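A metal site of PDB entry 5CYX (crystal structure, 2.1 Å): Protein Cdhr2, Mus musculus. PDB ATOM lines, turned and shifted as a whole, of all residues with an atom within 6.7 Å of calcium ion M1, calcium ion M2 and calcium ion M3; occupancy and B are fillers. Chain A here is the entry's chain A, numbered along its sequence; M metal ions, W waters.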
ATOM      1  N   GLU A  18     -20.800  36.371 -17.313  1.00  0.00           N
ATOM      2  CA  GLU A  18     -21.195  36.898 -16.020  1.00  0.00           C
ATOM      3  C   GLU A  18     -20.199  37.931 -15.459  1.00  0.00           C
ATOM      4  O   GLU A  18     -20.551  38.696 -14.654  1.00  0.00           O
ATOM      5  CB  GLU A  18     -21.438  35.758 -15.023  1.00  0.00           C
ATOM      6  CG  GLU A  18     -20.217  35.030 -14.456  1.00  0.00           C
ATOM      7  CD  GLU A  18     -20.517  34.246 -13.192  1.00  0.00           C
ATOM      8  OE1 GLU A  18     -21.360  34.704 -12.344  1.00  0.00           O
ATOM      9  OE2 GLU A  18     -19.890  33.174 -12.977  1.00  0.00           O
ATOM     10  N   LEU A  66     -24.457  40.839 -13.600  1.00  0.00           N
ATOM     11  CA  LEU A  66     -24.843  39.522 -13.967  1.00  0.00           C
ATOM     12  C   LEU A  66     -24.214  38.562 -12.985  1.00  0.00           C
ATOM     13  O   LEU A  66     -23.117  38.827 -12.495  1.00  0.00           O
ATOM     14  CB  LEU A  66     -24.272  39.179 -15.355  1.00  0.00           C
ATOM     15  CG  LEU A  66     -24.812  39.940 -16.551  1.00  0.00           C
ATOM     16  CD1 LEU A  66     -24.128  39.469 -17.828  1.00  0.00           C
ATOM     17  CD2 LEU A  66     -26.311  39.757 -16.693  1.00  0.00           C
ATOM     18  N   ASP A  67     -24.874  37.425 -12.761  1.00  0.00           N
ATOM     19  CA  ASP A  67     -24.380  36.470 -11.785  1.00  0.00           C
ATOM     20  C   ASP A  67     -24.971  35.113 -12.097  1.00  0.00           C
ATOM     21  O   ASP A  67     -26.142  34.838 -11.816  1.00  0.00           O
ATOM     22  CB  ASP A  67     -24.768  36.908 -10.324  1.00  0.00           C
ATOM     23  CG  ASP A  67     -24.199  35.955  -9.270  1.00  0.00           C
ATOM     24  OD1 ASP A  67     -23.264  35.161  -9.543  1.00  0.00           O
ATOM     25  OD2 ASP A  67     -24.697  35.941  -8.160  1.00  0.00           O
ATOM     26  N   PHE A  68     -24.159  34.261 -12.700  1.00  0.00           N
ATOM     27  CA  PHE A  68     -24.561  32.955 -13.093  1.00  0.00           C
ATOM     28  C   PHE A  68     -25.061  32.144 -11.915  1.00  0.00           C
ATOM     29  O   PHE A  68     -26.024  31.407 -12.047  1.00  0.00           O
ATOM     30  CB  PHE A  68     -23.378  32.199 -13.704  1.00  0.00           C
ATOM     31  CG  PHE A  68     -23.724  30.813 -14.114  1.00  0.00           C
ATOM     32  CD1 PHE A  68     -24.408  30.585 -15.295  1.00  0.00           C
ATOM     33  CD2 PHE A  68     -23.380  29.716 -13.320  1.00  0.00           C
ATOM     34  CE1 PHE A  68     -24.707  29.286 -15.696  1.00  0.00           C
ATOM     35  CE2 PHE A  68     -23.684  28.425 -13.710  1.00  0.00           C
ATOM     36  CZ  PHE A  68     -24.369  28.226 -14.877  1.00  0.00           C
ATOM     37  N   GLU A  69     -24.411  32.306 -10.762  1.00  0.00           N
ATOM     38  CA  GLU A  69     -24.769  31.518  -9.587  1.00  0.00           C
ATOM     39  C   GLU A  69     -26.216  31.745  -9.098  1.00  0.00           C
ATOM     40  O   GLU A  69     -26.807  30.813  -8.509  1.00  0.00           O
ATOM     41  CB  GLU A  69     -23.785  31.767  -8.443  1.00  0.00           C
ATOM     42  CG  GLU A  69     -22.493  30.987  -8.570  1.00  0.00           C
ATOM     43  CD  GLU A  69     -21.652  31.347  -9.809  1.00  0.00           C
ATOM     44  OE1 GLU A  69     -21.334  32.502 -10.083  1.00  0.00           O
ATOM     45  OE2 GLU A  69     -21.292  30.474 -10.555  1.00  0.00           O
ATOM     46  N   THR A  70     -26.806  32.919  -9.357  1.00  0.00           N
ATOM     47  CA  THR A  70     -28.221  33.198  -8.989  1.00  0.00           C
ATOM     48  C   THR A  70     -29.193  33.272 -10.162  1.00  0.00           C
ATOM     49  O   THR A  70     -30.295  32.750 -10.067  1.00  0.00           O
ATOM     50  CB  THR A  70     -28.374  34.497  -8.199  1.00  0.00           C
ATOM     51  OG1 THR A  70     -27.214  35.290  -8.431  1.00  0.00           O
ATOM     52  CG2 THR A  70     -28.469  34.250  -6.723  1.00  0.00           C
ATOM     53  N   GLU A  96     -23.273  33.204 -19.096  1.00  0.00           N
ATOM     54  CA  GLU A  96     -22.230  32.174 -18.997  1.00  0.00           C
ATOM     55  C   GLU A  96     -21.438  32.240 -17.689  1.00  0.00           C
ATOM     56  O   GLU A  96     -20.994  33.326 -17.231  1.00  0.00           O
ATOM     57  CB  GLU A  96     -21.238  32.283 -20.144  1.00  0.00           C
ATOM     58  CG  GLU A  96     -21.749  31.798 -21.477  1.00  0.00           C
ATOM     59  CD  GLU A  96     -20.629  31.615 -22.513  1.00  0.00           C
ATOM     60  OE1 GLU A  96     -19.650  32.406 -22.473  1.00  0.00           O
ATOM     61  OE2 GLU A  96     -20.779  30.682 -23.359  1.00  0.00           O
ATOM     62  N   ASP A  97     -21.189  31.057 -17.145  1.00  0.00           N
ATOM     63  CA  ASP A  97     -20.422  30.885 -15.929  1.00  0.00           C
ATOM     64  C   ASP A  97     -18.979  31.339 -16.172  1.00  0.00           C
ATOM     65  O   ASP A  97     -18.395  31.058 -17.253  1.00  0.00           O
ATOM     66  CB  ASP A  97     -20.431  29.397 -15.479  1.00  0.00           C
ATOM     67  CG  ASP A  97     -19.910  29.219 -14.033  1.00  0.00           C
ATOM     68  OD1 ASP A  97     -19.918  30.194 -13.232  1.00  0.00           O
ATOM     69  OD2 ASP A  97     -19.429  28.091 -13.725  1.00  0.00           O
ATOM     70  N   ARG A  98     -18.434  32.070 -15.196  1.00  0.00           N
ATOM     71  CA  ARG A  98     -16.948  32.340 -15.173  1.00  0.00           C
ATOM     72  C   ARG A  98     -16.402  31.993 -13.767  1.00  0.00           C
ATOM     73  O   ARG A  98     -17.181  31.894 -12.752  1.00  0.00           O
ATOM     74  CB  ARG A  98     -16.683  33.774 -15.556  1.00  0.00           C
ATOM     75  CG  ARG A  98     -17.033  34.133 -16.991  1.00  0.00           C
ATOM     76  CD  ARG A  98     -15.898  33.737 -17.892  1.00  0.00           C
ATOM     77  NE  ARG A  98     -16.177  33.965 -19.299  1.00  0.00           N
ATOM     78  CZ  ARG A  98     -16.824  33.151 -20.114  1.00  0.00           C
ATOM     79  NH1 ARG A  98     -16.979  33.482 -21.376  1.00  0.00           N
ATOM     80  NH2 ARG A  98     -17.327  31.995 -19.701  1.00  0.00           N
ATOM     81  N   ASN A  99     -15.094  31.763 -13.680  1.00  0.00           N
ATOM     82  CA  ASN A  99     -14.496  31.365 -12.428  1.00  0.00           C
ATOM     83  C   ASN A  99     -14.289  32.553 -11.462  1.00  0.00           C
ATOM     84  O   ASN A  99     -13.143  33.041 -11.284  1.00  0.00           O
ATOM     85  CB  ASN A  99     -13.197  30.625 -12.641  1.00  0.00           C
ATOM     86  CG  ASN A  99     -12.735  29.900 -11.441  1.00  0.00           C
ATOM     87  OD1 ASN A  99     -13.460  29.791 -10.452  1.00  0.00           O
ATOM     88  ND2 ASN A  99     -11.533  29.425 -11.495  1.00  0.00           N
ATOM     89  N   ASP A 100     -15.401  32.995 -10.861  1.00  0.00           N
ATOM     90  CA  ASP A 100     -15.386  34.092  -9.868  1.00  0.00           C
ATOM     91  C   ASP A 100     -15.654  33.564  -8.468  1.00  0.00           C
ATOM     92  O   ASP A 100     -15.806  34.356  -7.577  1.00  0.00           O
ATOM     93  CB  ASP A 100     -16.453  35.151 -10.209  1.00  0.00           C
ATOM     94  CG  ASP A 100     -17.902  34.539 -10.310  1.00  0.00           C
ATOM     95  OD1 ASP A 100     -18.063  33.312 -10.393  1.00  0.00           O
ATOM     96  OD2 ASP A 100     -18.884  35.279 -10.270  1.00  0.00           O
ATOM     97  N   ASN A 101     -15.788  32.235  -8.243  1.00  0.00           N
ATOM     98  CA  ASN A 101     -15.886  31.797  -6.828  1.00  0.00           C
ATOM     99  C   ASN A 101     -14.671  30.991  -6.392  1.00  0.00           C
ATOM    100  O   ASN A 101     -14.021  30.373  -7.247  1.00  0.00           O
ATOM    101  CB  ASN A 101     -17.172  31.052  -6.536  1.00  0.00           C
ATOM    102  CG  ASN A 101     -18.364  31.965  -6.506  1.00  0.00           C
ATOM    103  OD1 ASN A 101     -18.588  32.688  -5.517  1.00  0.00           O
ATOM    104  ND2 ASN A 101     -19.134  31.969  -7.564  1.00  0.00           N
ATOM    105  N   ILE A 102     -14.353  31.080  -5.082  1.00  0.00           N
ATOM    106  CA  ILE A 102     -13.296  30.256  -4.464  1.00  0.00           C
ATOM    107  C   ILE A 102     -13.828  29.025  -3.684  1.00  0.00           C
ATOM    108  O   ILE A 102     -14.986  29.013  -3.204  1.00  0.00           O
ATOM    109  CB  ILE A 102     -12.363  31.037  -3.536  1.00  0.00           C
ATOM    110  CG1 ILE A 102     -13.124  31.595  -2.295  1.00  0.00           C
ATOM    111  CG2 ILE A 102     -11.715  32.227  -4.243  1.00  0.00           C
ATOM    112  CD1 ILE A 102     -12.175  32.242  -1.293  1.00  0.00           C
ATOM    113  N   PRO A 103     -12.952  28.016  -3.512  1.00  0.00           N
ATOM    114  CA  PRO A 103     -13.260  26.912  -2.638  1.00  0.00           C
ATOM    115  C   PRO A 103     -13.309  27.386  -1.209  1.00  0.00           C
ATOM    116  O   PRO A 103     -12.396  28.057  -0.764  1.00  0.00           O
ATOM    117  CB  PRO A 103     -12.057  25.988  -2.835  1.00  0.00           C
ATOM    118  CG  PRO A 103     -11.594  26.256  -4.223  1.00  0.00           C
ATOM    119  CD  PRO A 103     -11.746  27.752  -4.315  1.00  0.00           C
ATOM    120  N   ASP A 131     -16.971  24.848  -3.942  1.00  0.00           N
ATOM    121  CA  ASP A 131     -16.760  25.978  -4.823  1.00  0.00           C
ATOM    122  C   ASP A 131     -18.006  26.087  -5.650  1.00  0.00           C
ATOM    123  O   ASP A 131     -18.362  25.146  -6.352  1.00  0.00           O
ATOM    124  CB  ASP A 131     -15.539  25.726  -5.713  1.00  0.00           C
ATOM    125  CG  ASP A 131     -15.194  26.907  -6.611  1.00  0.00           C
ATOM    126  OD1 ASP A 131     -16.056  27.484  -7.294  1.00  0.00           O
ATOM    127  OD2 ASP A 131     -13.985  27.236  -6.728  1.00  0.00           O
ATOM    128  N   LYS A 132     -18.652  27.245  -5.590  1.00  0.00           N
ATOM    129  CA  LYS A 132     -19.964  27.430  -6.230  1.00  0.00           C
ATOM    130  C   LYS A 132     -19.982  27.479  -7.753  1.00  0.00           C
ATOM    131  O   LYS A 132     -21.054  27.389  -8.331  1.00  0.00           O
ATOM    132  CB  LYS A 132     -20.625  28.676  -5.687  1.00  0.00           C
ATOM    133  CG  LYS A 132     -20.939  28.519  -4.206  1.00  0.00           C
ATOM    134  CD  LYS A 132     -22.374  28.910  -3.914  1.00  0.00           C
ATOM    135  CE  LYS A 132     -22.562  30.417  -3.898  1.00  0.00           C
ATOM    136  NZ  LYS A 132     -23.946  30.829  -4.338  1.00  0.00           N
ATOM    137  N   ASP A 133     -18.824  27.593  -8.406  1.00  0.00           N
ATOM    138  CA  ASP A 133     -18.829  27.636  -9.852  1.00  0.00           C
ATOM    139  C   ASP A 133     -19.155  26.211 -10.356  1.00  0.00           C
ATOM    140  O   ASP A 133     -19.188  25.263  -9.587  1.00  0.00           O
ATOM    141  CB  ASP A 133     -17.500  28.173 -10.428  1.00  0.00           C
ATOM    142  CG  ASP A 133     -17.168  29.574  -9.875  1.00  0.00           C
ATOM    143  OD1 ASP A 133     -18.081  30.445  -9.870  1.00  0.00           O
ATOM    144  OD2 ASP A 133     -16.065  29.693  -9.363  1.00  0.00           O
ATOM    145  N   THR A 134     -19.391  26.123 -11.669  1.00  0.00           N
ATOM    146  CA  THR A 134     -19.779  24.880 -12.341  1.00  0.00           C
ATOM    147  C   THR A 134     -18.674  24.474 -13.324  1.00  0.00           C
ATOM    148  O   THR A 134     -17.985  25.327 -13.865  1.00  0.00           O
ATOM    149  CB  THR A 134     -21.078  25.135 -13.116  1.00  0.00           C
ATOM    150  OG1 THR A 134     -22.139  25.465 -12.187  1.00  0.00           O
ATOM    151  CG2 THR A 134     -21.513  23.866 -13.949  1.00  0.00           C
ATOM    152  N   THR A 136     -14.997  22.796 -14.460  1.00  0.00           N
ATOM    153  CA  THR A 136     -13.679  22.696 -13.817  1.00  0.00           C
ATOM    154  C   THR A 136     -13.487  23.880 -12.891  1.00  0.00           C
ATOM    155  O   THR A 136     -12.716  23.799 -11.952  1.00  0.00           O
ATOM    156  CB  THR A 136     -12.517  22.624 -14.816  1.00  0.00           C
ATOM    157  OG1 THR A 136     -12.540  23.789 -15.616  1.00  0.00           O
ATOM    158  CG2 THR A 136     -12.707  21.352 -15.767  1.00  0.00           C
ATOM    159  N   ALA A 137     -14.157  24.981 -13.157  1.00  0.00           N
ATOM    160  CA  ALA A 137     -14.103  26.120 -12.238  1.00  0.00           C
ATOM    161  C   ALA A 137     -14.687  25.804 -10.884  1.00  0.00           C
ATOM    162  O   ALA A 137     -14.495  26.574  -9.902  1.00  0.00           O
ATOM    163  CB  ALA A 137     -14.852  27.284 -12.834  1.00  0.00           C
ATOM    164  N   GLY A 138     -15.506  24.734 -10.818  1.00  0.00           N
ATOM    165  CA  GLY A 138     -16.096  24.299  -9.573  1.00  0.00           C
ATOM    166  C   GLY A 138     -15.499  23.058  -8.946  1.00  0.00           C
ATOM    167  O   GLY A 138     -15.911  22.648  -7.889  1.00  0.00           O
ATOM    168  N   LEU A 139     -14.502  22.475  -9.583  1.00  0.00           N
ATOM    169  CA  LEU A 139     -14.018  21.150  -9.270  1.00  0.00           C
ATOM    170  C   LEU A 139     -12.787  21.320  -8.364  1.00  0.00           C
ATOM    171  O   LEU A 139     -11.687  21.802  -8.826  1.00  0.00           O
ATOM    172  CB  LEU A 139     -13.620  20.453 -10.563  1.00  0.00           C
ATOM    173  CG  LEU A 139     -13.268  18.967 -10.459  1.00  0.00           C
ATOM    174  CD1 LEU A 139     -14.442  18.185  -9.862  1.00  0.00           C
ATOM    175  CD2 LEU A 139     -12.935  18.430 -11.847  1.00  0.00           C
ATOM    176  N   ASP A 189      -9.609  25.296  -7.205  1.00  0.00           N
ATOM    177  CA  ASP A 189     -10.424  24.714  -8.225  1.00  0.00           C
ATOM    178  C   ASP A 189      -9.456  24.228  -9.338  1.00  0.00           C
ATOM    179  O   ASP A 189      -8.212  24.423  -9.259  1.00  0.00           O
ATOM    180  CB  ASP A 189     -11.550  25.658  -8.702  1.00  0.00           C
ATOM    181  CG  ASP A 189     -11.055  26.991  -9.198  1.00  0.00           C
ATOM    182  OD1 ASP A 189      -9.967  27.033  -9.788  1.00  0.00           O
ATOM    183  OD2 ASP A 189     -11.739  28.027  -8.946  1.00  0.00           O
ATOM    184  N   SER A 190     -10.030  23.696 -10.378  1.00  0.00           N
ATOM    185  CA  SER A 190      -9.285  23.075 -11.474  1.00  0.00           C
ATOM    186  C   SER A 190      -9.220  24.048 -12.675  1.00  0.00           C
ATOM    187  O   SER A 190      -8.944  23.676 -13.780  1.00  0.00           O
ATOM    188  CB  SER A 190      -9.965  21.738 -11.850  1.00  0.00           C
ATOM    189  OG  SER A 190     -10.127  20.868 -10.734  1.00  0.00           O
ATOM    190  N   THR A 200      -7.377  30.250 -11.970  1.00  0.00           N
ATOM    191  CA  THR A 200      -7.573  29.197 -10.963  1.00  0.00           C
ATOM    192  C   THR A 200      -7.776  29.913  -9.647  1.00  0.00           C
ATOM    193  O   THR A 200      -7.025  30.849  -9.365  1.00  0.00           O
ATOM    194  CB  THR A 200      -6.332  28.291 -10.864  1.00  0.00           C
ATOM    195  OG1 THR A 200      -6.168  27.534 -12.090  1.00  0.00           O
ATOM    196  CG2 THR A 200      -6.439  27.346  -9.656  1.00  0.00           C
ATOM    197  N   GLN A 201      -8.755  29.504  -8.839  1.00  0.00           N
ATOM    198  CA  GLN A 201      -8.950  30.165  -7.506  1.00  0.00           C
ATOM    199  C   GLN A 201      -8.544  29.254  -6.375  1.00  0.00           C
ATOM    200  O   GLN A 201      -8.766  28.033  -6.461  1.00  0.00           O
ATOM    201  CB  GLN A 201     -10.394  30.580  -7.322  1.00  0.00           C
ATOM    202  CG  GLN A 201     -10.933  31.495  -8.400  1.00  0.00           C
ATOM    203  CD  GLN A 201     -10.713  32.965  -8.119  1.00  0.00           C
ATOM    204  OE1 GLN A 201     -10.027  33.333  -7.168  1.00  0.00           O
ATOM    205  NE2 GLN A 201     -11.305  33.801  -8.941  1.00  0.00           N
HETATM  206 CA    CA M   1     -21.017  34.906  -9.993  1.00  0.00          CA
HETATM  207 CA    CA M   2     -19.277  31.638 -11.527  1.00  0.00          CA
HETATM  208 CA    CA M   3     -14.168  28.526  -8.652  1.00  0.00          CA
HETATM  209  O   HOH W   1     -20.464  34.937  -7.598  1.00  0.00           O
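Four residues have an atom within 4 Å of calcium ion M1: Glu 18, Asp 67, Glu 69 and Asp 100. The nearest printed residue that does not touch calcium ion M1 is Phe 68 (4.2 Å).
Calcium ion M1 is bound by OD2 of Asp 100 (2.2 Å), OD1 of Asp 67 (2.3 Å), OE1 of Glu 18 (2.4 Å), OE1 of Glu 69 (2.4 Å) and water W1 (2.5 Å). Calcium ion M1 has five donor atoms within binding distance.
OG1 of Thr 70 sits at hydrogen-bond distance from OD2 of Asp 67 (2.6 Å). NH1 of Arg 98 lies within salt-bridge range of OE1 of Glu 96 (3.1 Å). OE1 of Glu 69 sits close to ND2 of Asn 101 (3.4 Å). The side-chain amide nitrogen of Asn 101 sits close to the side-chain carboxylate of Asp 100 (3.3 Å). The backbone carbonyl oxygen (O) of Asn 99 sits at hydrogen-bond distance from the side-chain amide nitrogen (NE2) of Gln 201 (3.1 Å). The backbone NH of Gln 201 lies within hydrogen-bond range of the side-chain carboxylate of Asp 189 (2.9 Å). OD2 of Asp 97 lies within hydrogen-bond range of N of Thr 134, 2.8 Å away. OE1 of Glu 18 sits close to N of Phe 68.
Calcium ion M2 is bound by OE2 of Glu 18 (2.2 Å), OD1 of Asp 97 (2.3 Å), OD1 of Asp 100 (2.4 Å), OD1 of Asp 133 (2.4 Å), O of Arg 98 (2.4 Å), OE2 of Glu 69 (2.5 Å) and OE1 of Glu 69 (2.7 Å).
Calcium ion M3 is bound by the side-chain amide oxygen (OD1) of Asn 99, at 2.3 Å. The side-chain carboxylate (OD2) of Asp 131 binds calcium ion M3. O of Asn 101 binds calcium ion M3 (2.3 Å). OD2 of Asp 133 binds calcium ion M3 (2.3 Å). O of Ala 137 is bound to calcium ion M3 (2.3 Å). OD2 of Asp 189 binds calcium ion M3 (2.5 Å). OD1 of Asp 131 binds calcium ion M3 (2.5 Å). Calcium ion M3 has seven donor atoms within binding distance.
Six residues have an atom within 4 Å of calcium ion M3: Asn 99, Asn 101, Asp 131, Asp 133, Ala 137 and Asp 189. The nearest printed residue that does not touch calcium ion M3 is Ile 102 (4.4 Å).
Of the 26 residues printed, 7 come within 4 Å of calcium ion M2. The nearest printed residue that does not touch calcium ion M2 is Phe 68 (4.7 Å).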
